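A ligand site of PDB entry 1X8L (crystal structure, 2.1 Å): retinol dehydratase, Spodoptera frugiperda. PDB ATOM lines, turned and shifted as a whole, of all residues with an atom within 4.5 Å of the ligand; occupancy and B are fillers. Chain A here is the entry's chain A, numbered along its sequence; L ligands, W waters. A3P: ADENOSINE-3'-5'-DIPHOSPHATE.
The backbone carbonyl oxygen (O) of Leu 282 sits at hydrogen-bond distance from a nitrogen (N6) of the ligand (2.9 Å). O2P of the ligand is in hydrogen-bond range of N of Gly 314, at 3.0 Å. The guanidinium group of Arg 312 lies within salt-bridge range of an oxygen (O1P) of the ligand. The backbone NH of Ser 74 lies within hydrogen-bond range of an oxygen (O5P) of the ligand (3.2 Å). The side-chain hydroxyl (OG) of Ser 193 lies within hydrogen-bond range of an oxygen (O1P) of the ligand (2.6 Å). An oxygen (O5P) of the ligand lies within hydrogen-bond range of the backbone NH (N) of Arg 73, at 3.3 Å. The backbone NH (N) of Thr 77 sits at hydrogen-bond distance from an oxygen (O4P) of the ligand. The guanidinium group of Arg 185 is in salt-bridge range of an oxygen (O3P) of the ligand (2.8 Å). N of Gly 75 lies within hydrogen-bond range of O5' of the ligand. An oxygen (O6P) of the ligand is in salt-bridge range of the guanidinium group (NH1) of Arg 73 (2.7 Å). OH of Tyr 248 lies within hydrogen-bond range of N3 of the ligand. N of Thr 76 lies within hydrogen-bond range of O5P of the ligand, at 2.7 Å. O5P of the ligand lies within hydrogen-bond range of OG1 of Thr 76 (2.6 Å). N of Arg 312 sits at hydrogen-bond distance from O2' of the ligand, 3.1 Å away. O2P of the ligand lies within hydrogen-bond range of N of Lys 313, at 2.8 Å. The side-chain hydroxyl (OG1) of Thr 77 sits at hydrogen-bond distance from an oxygen (O4P) of the ligand (2.6 Å).
O of Lys 315 is in hydrogen-bond range of NH2 of Arg 185 (3.1 Å). OG1 of Thr 76 is in hydrogen-bond range of OG of Ser 70 (2.6 Å). The backbone carbonyl oxygen (O) of Gln 72 is in hydrogen-bond range of the side-chain hydroxyl (OG) of Ser 74 (3.5 Å). OG of Ser 193 is in hydrogen-bond range of NE of Arg 73, 2.8 Å away. O of Arg 73 lies within hydrogen-bond range of NH1 of Arg 185 (2.8 Å). The guanidinium group of Arg 73 lies within hydrogen-bond range of the backbone carbonyl oxygen of Phe 310, at 2.9 Å.
SD of Met 78 lies close to N1 of the ligand. Merely in contact with the ligand: Phe 284 (3.5 Å), Phe 287 (3.3 Å) and Ile 311 (3.6 Å). Hydrophobic or aromatic side chains within 4 Å of the ligand: Met 78, Tyr 248, Leu 282, Phe 284, Phe 287 and Ile 311. Within 4 Å of the ligand: Arg 73, Ser 74, Gly 75, Thr 76, Thr 77, Met 78, Arg 185, Ser 193, Tyr 248, Leu 282, Phe 284, Phe 287, Ile 311, Arg 312, Lys 313 and Gly 314.
Water W3 lies within hydrogen-bond range of an oxygen (O3P) of the ligand (2.7 Å) and the guanidinium group of Arg 312 (3.1 Å). Water W4 bridges an oxygen (O6P) of the ligand (2.7 Å) and the backbone NH (N) of Arg 73 (3.3 Å). Water W6 lies within hydrogen-bond range of an oxygen (O4P) of the ligand (2.7 Å), the backbone NH of Met 78 (3.2 Å) and the backbone NH of Thr 77 (3.3 Å). Water W1 bridges O3P of the ligand (2.8 Å) and N of Lys 315 (3.1 Å). Water W2 lies within hydrogen-bond range of the backbone carbonyl oxygen (O) of Phe 310, an oxygen (O4P) of the ligand and the side-chain hydroxyl (OG1) of Thr 77. Water W5 lies within hydrogen-bond range of the guanidinium group of Arg 73, the backbone carbonyl oxygen of Ser 193, the guanidinium group of Arg 312 and an oxygen (O1P) of the ligand.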
ATOM      1  N   SER A  70       6.106 -27.862 -30.188  1.00  0.00           N
ATOM      2  CA  SER A  70       5.935 -26.514 -30.706  1.00  0.00           C
ATOM      3  C   SER A  70       6.390 -26.476 -32.153  1.00  0.00           C
ATOM      4  O   SER A  70       7.245 -27.251 -32.545  1.00  0.00           O
ATOM      5  CB  SER A  70       6.820 -25.499 -29.994  1.00  0.00           C
ATOM      6  OG  SER A  70       8.187 -25.823 -30.186  1.00  0.00           O
ATOM      7  N   GLN A  72       8.972 -24.455 -33.981  1.00  0.00           N
ATOM      8  CA  GLN A  72      10.213 -23.939 -33.412  1.00  0.00           C
ATOM      9  C   GLN A  72      10.214 -22.419 -33.165  1.00  0.00           C
ATOM     10  O   GLN A  72       9.474 -21.644 -33.820  1.00  0.00           O
ATOM     11  CB  GLN A  72      11.415 -24.294 -34.305  1.00  0.00           C
ATOM     12  CG  GLN A  72      11.296 -23.886 -35.826  1.00  0.00           C
ATOM     13  CD  GLN A  72      12.494 -24.385 -36.626  1.00  0.00           C
ATOM     14  OE1 GLN A  72      13.605 -23.995 -36.389  1.00  0.00           O
ATOM     15  NE2 GLN A  72      12.257 -25.264 -37.573  1.00  0.00           N
ATOM     16  N   ARG A  73      11.038 -22.037 -32.214  1.00  0.00           N
ATOM     17  CA  ARG A  73      11.243 -20.656 -31.803  1.00  0.00           C
ATOM     18  C   ARG A  73      10.020 -20.027 -31.141  1.00  0.00           C
ATOM     19  O   ARG A  73       9.790 -18.834 -31.299  1.00  0.00           O
ATOM     20  CB  ARG A  73      11.771 -19.819 -32.962  1.00  0.00           C
ATOM     21  CG  ARG A  73      12.968 -20.417 -33.682  1.00  0.00           C
ATOM     22  CD  ARG A  73      14.065 -20.861 -32.729  1.00  0.00           C
ATOM     23  NE  ARG A  73      14.818 -19.724 -32.216  1.00  0.00           N
ATOM     24  CZ  ARG A  73      15.673 -19.752 -31.207  1.00  0.00           C
ATOM     25  NH1 ARG A  73      15.912 -20.886 -30.502  1.00  0.00           N
ATOM     26  NH2 ARG A  73      16.318 -18.652 -30.906  1.00  0.00           N
ATOM     27  N   SER A  74       9.253 -20.856 -30.417  1.00  0.00           N
ATOM     28  CA  SER A  74       7.966 -20.458 -29.858  1.00  0.00           C
ATOM     29  C   SER A  74       7.950 -20.595 -28.324  1.00  0.00           C
ATOM     30  O   SER A  74       6.877 -20.517 -27.705  1.00  0.00           O
ATOM     31  CB  SER A  74       6.834 -21.336 -30.465  1.00  0.00           C
ATOM     32  OG  SER A  74       6.640 -21.126 -31.866  1.00  0.00           O
ATOM     33  N   GLY A  75       9.136 -20.832 -27.715  1.00  0.00           N
ATOM     34  CA  GLY A  75       9.258 -21.009 -26.261  1.00  0.00           C
ATOM     35  C   GLY A  75       9.508 -22.437 -25.763  1.00  0.00           C
ATOM     36  O   GLY A  75       9.255 -22.768 -24.584  1.00  0.00           O
ATOM     37  N   THR A  76       9.990 -23.308 -26.650  1.00  0.00           N
ATOM     38  CA  THR A  76      10.290 -24.698 -26.262  1.00  0.00           C
ATOM     39  C   THR A  76      11.296 -24.828 -25.087  1.00  0.00           C
ATOM     40  O   THR A  76      11.042 -25.547 -24.112  1.00  0.00           O
ATOM     41  CB  THR A  76      10.862 -25.485 -27.446  1.00  0.00           C
ATOM     42  OG1 THR A  76      10.174 -25.138 -28.664  1.00  0.00           O
ATOM     43  CG2 THR A  76      10.600 -26.981 -27.256  1.00  0.00           C
ATOM     44  N   THR A  77      12.422 -24.137 -25.192  1.00  0.00           N
ATOM     45  CA  THR A  77      13.518 -24.307 -24.225  1.00  0.00           C
ATOM     46  C   THR A  77      13.126 -23.886 -22.830  1.00  0.00           C
ATOM     47  O   THR A  77      13.479 -24.559 -21.875  1.00  0.00           O
ATOM     48  CB  THR A  77      14.743 -23.489 -24.634  1.00  0.00           C
ATOM     49  OG1 THR A  77      15.109 -23.781 -25.972  1.00  0.00           O
ATOM     50  CG2 THR A  77      15.985 -23.922 -23.809  1.00  0.00           C
ATOM     51  N   MET A  78      12.418 -22.757 -22.724  1.00  0.00           N
ATOM     52  CA  MET A  78      11.864 -22.250 -21.470  1.00  0.00           C
ATOM     53  C   MET A  78      10.984 -23.317 -20.841  1.00  0.00           C
ATOM     54  O   MET A  78      11.072 -23.583 -19.657  1.00  0.00           O
ATOM     55  CB  MET A  78      10.958 -21.024 -21.718  1.00  0.00           C
ATOM     56  CG  MET A  78      11.648 -19.785 -22.135  1.00  0.00           C
ATOM     57  SD  MET A  78      10.435 -18.588 -22.584  1.00  0.00           S
ATOM     58  CE  MET A  78       9.794 -18.190 -21.007  1.00  0.00           C
ATOM     59  N   ARG A 185       3.190 -19.104 -30.701  1.00  0.00           N
ATOM     60  CA  ARG A 185       3.732 -17.772 -30.664  1.00  0.00           C
ATOM     61  C   ARG A 185       3.365 -17.055 -31.972  1.00  0.00           C
ATOM     62  O   ARG A 185       3.259 -17.657 -33.048  1.00  0.00           O
ATOM     63  CB  ARG A 185       5.247 -17.866 -30.519  1.00  0.00           C
ATOM     64  CG  ARG A 185       5.949 -16.546 -30.406  1.00  0.00           C
ATOM     65  CD  ARG A 185       7.476 -16.669 -30.456  1.00  0.00           C
ATOM     66  NE  ARG A 185       8.118 -15.409 -30.136  1.00  0.00           N
ATOM     67  CZ  ARG A 185       9.432 -15.232 -30.054  1.00  0.00           C
ATOM     68  NH1 ARG A 185      10.272 -16.234 -30.306  1.00  0.00           N
ATOM     69  NH2 ARG A 185       9.890 -14.036 -29.717  1.00  0.00           N
ATOM     70  N   SER A 193      12.664 -15.119 -35.425  1.00  0.00           N
ATOM     71  CA  SER A 193      13.516 -15.900 -34.597  1.00  0.00           C
ATOM     72  C   SER A 193      14.067 -17.070 -35.397  1.00  0.00           C
ATOM     73  O   SER A 193      15.232 -17.405 -35.206  1.00  0.00           O
ATOM     74  CB  SER A 193      12.799 -16.399 -33.328  1.00  0.00           C
ATOM     75  OG  SER A 193      13.755 -17.105 -32.561  1.00  0.00           O
ATOM     76  N   TYR A 248       3.640 -18.338 -25.925  1.00  0.00           N
ATOM     77  CA  TYR A 248       4.904 -17.693 -25.562  1.00  0.00           C
ATOM     78  C   TYR A 248       4.709 -16.358 -24.881  1.00  0.00           C
ATOM     79  O   TYR A 248       5.439 -16.032 -23.951  1.00  0.00           O
ATOM     80  CB  TYR A 248       5.766 -17.481 -26.811  1.00  0.00           C
ATOM     81  CG  TYR A 248       7.069 -16.753 -26.526  1.00  0.00           C
ATOM     82  CD1 TYR A 248       8.158 -17.416 -25.944  1.00  0.00           C
ATOM     83  CD2 TYR A 248       7.194 -15.393 -26.818  1.00  0.00           C
ATOM     84  CE1 TYR A 248       9.345 -16.732 -25.656  1.00  0.00           C
ATOM     85  CE2 TYR A 248       8.360 -14.716 -26.552  1.00  0.00           C
ATOM     86  CZ  TYR A 248       9.434 -15.374 -25.954  1.00  0.00           C
ATOM     87  OH  TYR A 248      10.581 -14.657 -25.693  1.00  0.00           O
ATOM     88  N   LEU A 252       5.804 -13.876 -21.093  1.00  0.00           N
ATOM     89  CA  LEU A 252       6.199 -12.474 -20.977  1.00  0.00           C
ATOM     90  C   LEU A 252       5.242 -11.633 -20.124  1.00  0.00           C
ATOM     91  O   LEU A 252       5.689 -10.769 -19.393  1.00  0.00           O
ATOM     92  CB  LEU A 252       6.336 -11.839 -22.383  1.00  0.00           C
ATOM     93  CG  LEU A 252       7.394 -12.515 -23.286  1.00  0.00           C
ATOM     94  CD1 LEU A 252       7.735 -11.676 -24.493  1.00  0.00           C
ATOM     95  CD2 LEU A 252       8.683 -12.871 -22.505  1.00  0.00           C
ATOM     96  N   LEU A 282      14.010 -18.422 -14.751  1.00  0.00           N
ATOM     97  CA  LEU A 282      13.708 -18.139 -16.160  1.00  0.00           C
ATOM     98  C   LEU A 282      13.833 -16.680 -16.576  1.00  0.00           C
ATOM     99  O   LEU A 282      13.526 -16.352 -17.722  1.00  0.00           O
ATOM    100  CB  LEU A 282      12.294 -18.656 -16.569  1.00  0.00           C
ATOM    101  CG  LEU A 282      12.156 -20.135 -16.974  1.00  0.00           C
ATOM    102  CD1 LEU A 282      12.709 -20.392 -18.336  1.00  0.00           C
ATOM    103  CD2 LEU A 282      12.841 -21.044 -15.962  1.00  0.00           C
ATOM    104  N   ASN A 283      14.253 -15.792 -15.679  1.00  0.00           N
ATOM    105  CA  ASN A 283      14.647 -14.438 -16.058  1.00  0.00           C
ATOM    106  C   ASN A 283      15.501 -14.490 -17.326  1.00  0.00           C
ATOM    107  O   ASN A 283      16.392 -15.342 -17.440  1.00  0.00           O
ATOM    108  CB  ASN A 283      15.428 -13.807 -14.900  1.00  0.00           C
ATOM    109  CG  ASN A 283      16.021 -12.440 -15.242  1.00  0.00           C
ATOM    110  OD1 ASN A 283      17.100 -12.364 -15.807  1.00  0.00           O
ATOM    111  ND2 ASN A 283      15.339 -11.358 -14.858  1.00  0.00           N
ATOM    112  N   PHE A 284      15.233 -13.620 -18.294  1.00  0.00           N
ATOM    113  CA  PHE A 284      15.889 -13.749 -19.590  1.00  0.00           C
ATOM    114  C   PHE A 284      17.414 -13.686 -19.500  1.00  0.00           C
ATOM    115  O   PHE A 284      18.085 -14.570 -20.000  1.00  0.00           O
ATOM    116  CB  PHE A 284      15.402 -12.704 -20.613  1.00  0.00           C
ATOM    117  CG  PHE A 284      15.918 -12.955 -22.022  1.00  0.00           C
ATOM    118  CD1 PHE A 284      15.316 -13.921 -22.832  1.00  0.00           C
ATOM    119  CD2 PHE A 284      16.986 -12.224 -22.535  1.00  0.00           C
ATOM    120  CE1 PHE A 284      15.783 -14.151 -24.126  1.00  0.00           C
ATOM    121  CE2 PHE A 284      17.446 -12.456 -23.822  1.00  0.00           C
ATOM    122  CZ  PHE A 284      16.837 -13.414 -24.623  1.00  0.00           C
ATOM    123  N   PHE A 287      18.936 -16.869 -17.798  1.00  0.00           N
ATOM    124  CA  PHE A 287      18.738 -18.038 -18.670  1.00  0.00           C
ATOM    125  C   PHE A 287      19.663 -18.009 -19.903  1.00  0.00           C
ATOM    126  O   PHE A 287      20.243 -19.012 -20.272  1.00  0.00           O
ATOM    127  CB  PHE A 287      17.251 -18.086 -19.143  1.00  0.00           C
ATOM    128  CG  PHE A 287      16.735 -19.470 -19.496  1.00  0.00           C
ATOM    129  CD1 PHE A 287      16.608 -20.443 -18.522  1.00  0.00           C
ATOM    130  CD2 PHE A 287      16.340 -19.763 -20.804  1.00  0.00           C
ATOM    131  CE1 PHE A 287      16.116 -21.725 -18.861  1.00  0.00           C
ATOM    132  CE2 PHE A 287      15.861 -21.031 -21.155  1.00  0.00           C
ATOM    133  CZ  PHE A 287      15.749 -22.012 -20.184  1.00  0.00           C
ATOM    134  N   PHE A 310      21.466 -18.678 -29.470  1.00  0.00           N
ATOM    135  CA  PHE A 310      20.278 -19.514 -29.342  1.00  0.00           C
ATOM    136  C   PHE A 310      19.222 -18.911 -28.390  1.00  0.00           C
ATOM    137  O   PHE A 310      18.002 -19.067 -28.616  1.00  0.00           O
ATOM    138  CB  PHE A 310      20.697 -20.939 -28.924  1.00  0.00           C
ATOM    139  CG  PHE A 310      19.557 -21.906 -28.833  1.00  0.00           C
ATOM    140  CD1 PHE A 310      19.027 -22.494 -29.979  1.00  0.00           C
ATOM    141  CD2 PHE A 310      19.014 -22.245 -27.604  1.00  0.00           C
ATOM    142  CE1 PHE A 310      17.995 -23.397 -29.895  1.00  0.00           C
ATOM    143  CE2 PHE A 310      17.967 -23.150 -27.519  1.00  0.00           C
ATOM    144  CZ  PHE A 310      17.442 -23.717 -28.669  1.00  0.00           C
ATOM    145  N   ILE A 311      19.665 -18.266 -27.306  1.00  0.00           N
ATOM    146  CA  ILE A 311      18.790 -17.395 -26.509  1.00  0.00           C
ATOM    147  C   ILE A 311      19.190 -15.979 -26.933  1.00  0.00           C
ATOM    148  O   ILE A 311      20.306 -15.574 -26.671  1.00  0.00           O
ATOM    149  CB  ILE A 311      18.992 -17.573 -24.965  1.00  0.00           C
ATOM    150  CG1 ILE A 311      19.089 -19.052 -24.543  1.00  0.00           C
ATOM    151  CG2 ILE A 311      17.922 -16.827 -24.206  1.00  0.00           C
ATOM    152  CD1 ILE A 311      17.850 -19.795 -24.631  1.00  0.00           C
ATOM    153  N   ARG A 312      18.283 -15.227 -27.555  1.00  0.00           N
ATOM    154  CA  ARG A 312      18.630 -14.080 -28.380  1.00  0.00           C
ATOM    155  C   ARG A 312      18.170 -12.701 -27.836  1.00  0.00           C
ATOM    156  O   ARG A 312      18.995 -11.876 -27.465  1.00  0.00           O
ATOM    157  CB  ARG A 312      18.083 -14.310 -29.812  1.00  0.00           C
ATOM    158  CG  ARG A 312      18.592 -13.341 -30.878  1.00  0.00           C
ATOM    159  CD  ARG A 312      18.069 -13.589 -32.264  1.00  0.00           C
ATOM    160  NE  ARG A 312      16.596 -13.543 -32.356  1.00  0.00           N
ATOM    161  CZ  ARG A 312      15.875 -12.426 -32.535  1.00  0.00           C
ATOM    162  NH1 ARG A 312      16.458 -11.243 -32.648  1.00  0.00           N
ATOM    163  NH2 ARG A 312      14.565 -12.487 -32.578  1.00  0.00           N
ATOM    164  N   LYS A 313      16.870 -12.447 -27.814  1.00  0.00           N
ATOM    165  CA  LYS A 313      16.370 -11.159 -27.295  1.00  0.00           C
ATOM    166  C   LYS A 313      15.269 -11.319 -26.254  1.00  0.00           C
ATOM    167  O   LYS A 313      15.305 -10.666 -25.215  1.00  0.00           O
ATOM    168  CB  LYS A 313      15.913 -10.223 -28.421  1.00  0.00           C
ATOM    169  CG  LYS A 313      16.989  -9.824 -29.438  1.00  0.00           C
ATOM    170  CD  LYS A 313      17.976  -8.744 -28.934  1.00  0.00           C
ATOM    171  CE  LYS A 313      19.114  -8.531 -29.965  1.00  0.00           C
ATOM    172  NZ  LYS A 313      20.088  -7.493 -29.555  1.00  0.00           N
ATOM    173  N   GLY A 314      14.283 -12.152 -26.526  1.00  0.00           N
ATOM    174  CA  GLY A 314      13.288 -12.503 -25.502  1.00  0.00           C
ATOM    175  C   GLY A 314      12.076 -11.585 -25.417  1.00  0.00           C
ATOM    176  O   GLY A 314      11.455 -11.512 -24.373  1.00  0.00           O
ATOM    177  N   LYS A 315      11.754 -10.906 -26.524  1.00  0.00           N
ATOM    178  CA  LYS A 315      10.685  -9.908 -26.602  1.00  0.00           C
ATOM    179  C   LYS A 315       9.532 -10.382 -27.470  1.00  0.00           C
ATOM    180  O   LYS A 315       9.675 -11.321 -28.246  1.00  0.00           O
ATOM    181  CB  LYS A 315      11.212  -8.591 -27.219  1.00  0.00           C
ATOM    182  CG  LYS A 315      12.397  -7.924 -26.515  1.00  0.00           C
ATOM    183  CD  LYS A 315      12.093  -7.586 -25.076  1.00  0.00           C
ATOM    184  CE  LYS A 315      13.245  -6.884 -24.406  1.00  0.00           C
ATOM    185  NZ  LYS A 315      12.925  -6.655 -22.946  1.00  0.00           N
HETATM  186  P1  A3P L   1      13.738 -14.734 -29.827  1.00  0.00           P
HETATM  187  O1P A3P L   1      14.555 -15.160 -31.049  1.00  0.00           O
HETATM  188  O2P A3P L   1      14.735 -14.025 -28.837  1.00  0.00           O
HETATM  189  O3P A3P L   1      12.555 -13.846 -30.400  1.00  0.00           O
HETATM  190  P2  A3P L   1      12.587 -22.079 -28.667  1.00  0.00           P
HETATM  191  O4P A3P L   1      13.191 -22.536 -27.309  1.00  0.00           O
HETATM  192  O5P A3P L   1      11.282 -22.865 -29.014  1.00  0.00           O
HETATM  193  O6P A3P L   1      13.650 -22.254 -29.790  1.00  0.00           O
HETATM  194  O5' A3P L   1      12.213 -20.522 -28.480  1.00  0.00           O
HETATM  195  C5' A3P L   1      13.174 -19.533 -28.804  1.00  0.00           C
HETATM  196  C4' A3P L   1      12.722 -18.131 -28.415  1.00  0.00           C
HETATM  197  O4' A3P L   1      12.425 -18.079 -27.030  1.00  0.00           O
HETATM  198  C3' A3P L   1      13.890 -17.210 -28.662  1.00  0.00           C
HETATM  199  O3' A3P L   1      13.175 -15.983 -28.970  1.00  0.00           O
HETATM  200  C2' A3P L   1      14.497 -16.901 -27.332  1.00  0.00           C
HETATM  201  O2' A3P L   1      15.273 -15.734 -27.182  1.00  0.00           O
HETATM  202  C1' A3P L   1      13.342 -17.178 -26.393  1.00  0.00           C
HETATM  203  N9  A3P L   1      13.673 -17.471 -25.017  1.00  0.00           N
HETATM  204  C8  A3P L   1      14.460 -18.467 -24.556  1.00  0.00           C
HETATM  205  N7  A3P L   1      14.500 -18.437 -23.199  1.00  0.00           N
HETATM  206  C5  A3P L   1      13.768 -17.415 -22.796  1.00  0.00           C
HETATM  207  C6  A3P L   1      13.365 -16.782 -21.530  1.00  0.00           C
HETATM  208  N6  A3P L   1      13.865 -17.329 -20.425  1.00  0.00           N
HETATM  209  N1  A3P L   1      12.526 -15.723 -21.541  1.00  0.00           N
HETATM  210  C2  A3P L   1      12.031 -15.168 -22.681  1.00  0.00           C
HETATM  211  N3  A3P L   1      12.329 -15.659 -23.891  1.00  0.00           N
HETATM  212  C4  A3P L   1      13.217 -16.806 -23.973  1.00  0.00           C
HETATM  213  O   HOH W   1      12.512 -11.148 -29.491  1.00  0.00           O
HETATM  214  O   HOH W   2      15.912 -20.546 -26.973  1.00  0.00           O
HETATM  215  O   HOH W   3      11.499 -12.980 -32.677  1.00  0.00           O
HETATM  216  O   HOH W   4      13.194 -24.421 -31.301  1.00  0.00           O
HETATM  217  O   HOH W   5      16.835 -16.801 -32.959  1.00  0.00           O
HETATM  218  O   HOH W   6      12.367 -20.846 -25.323  1.00  0.00           O
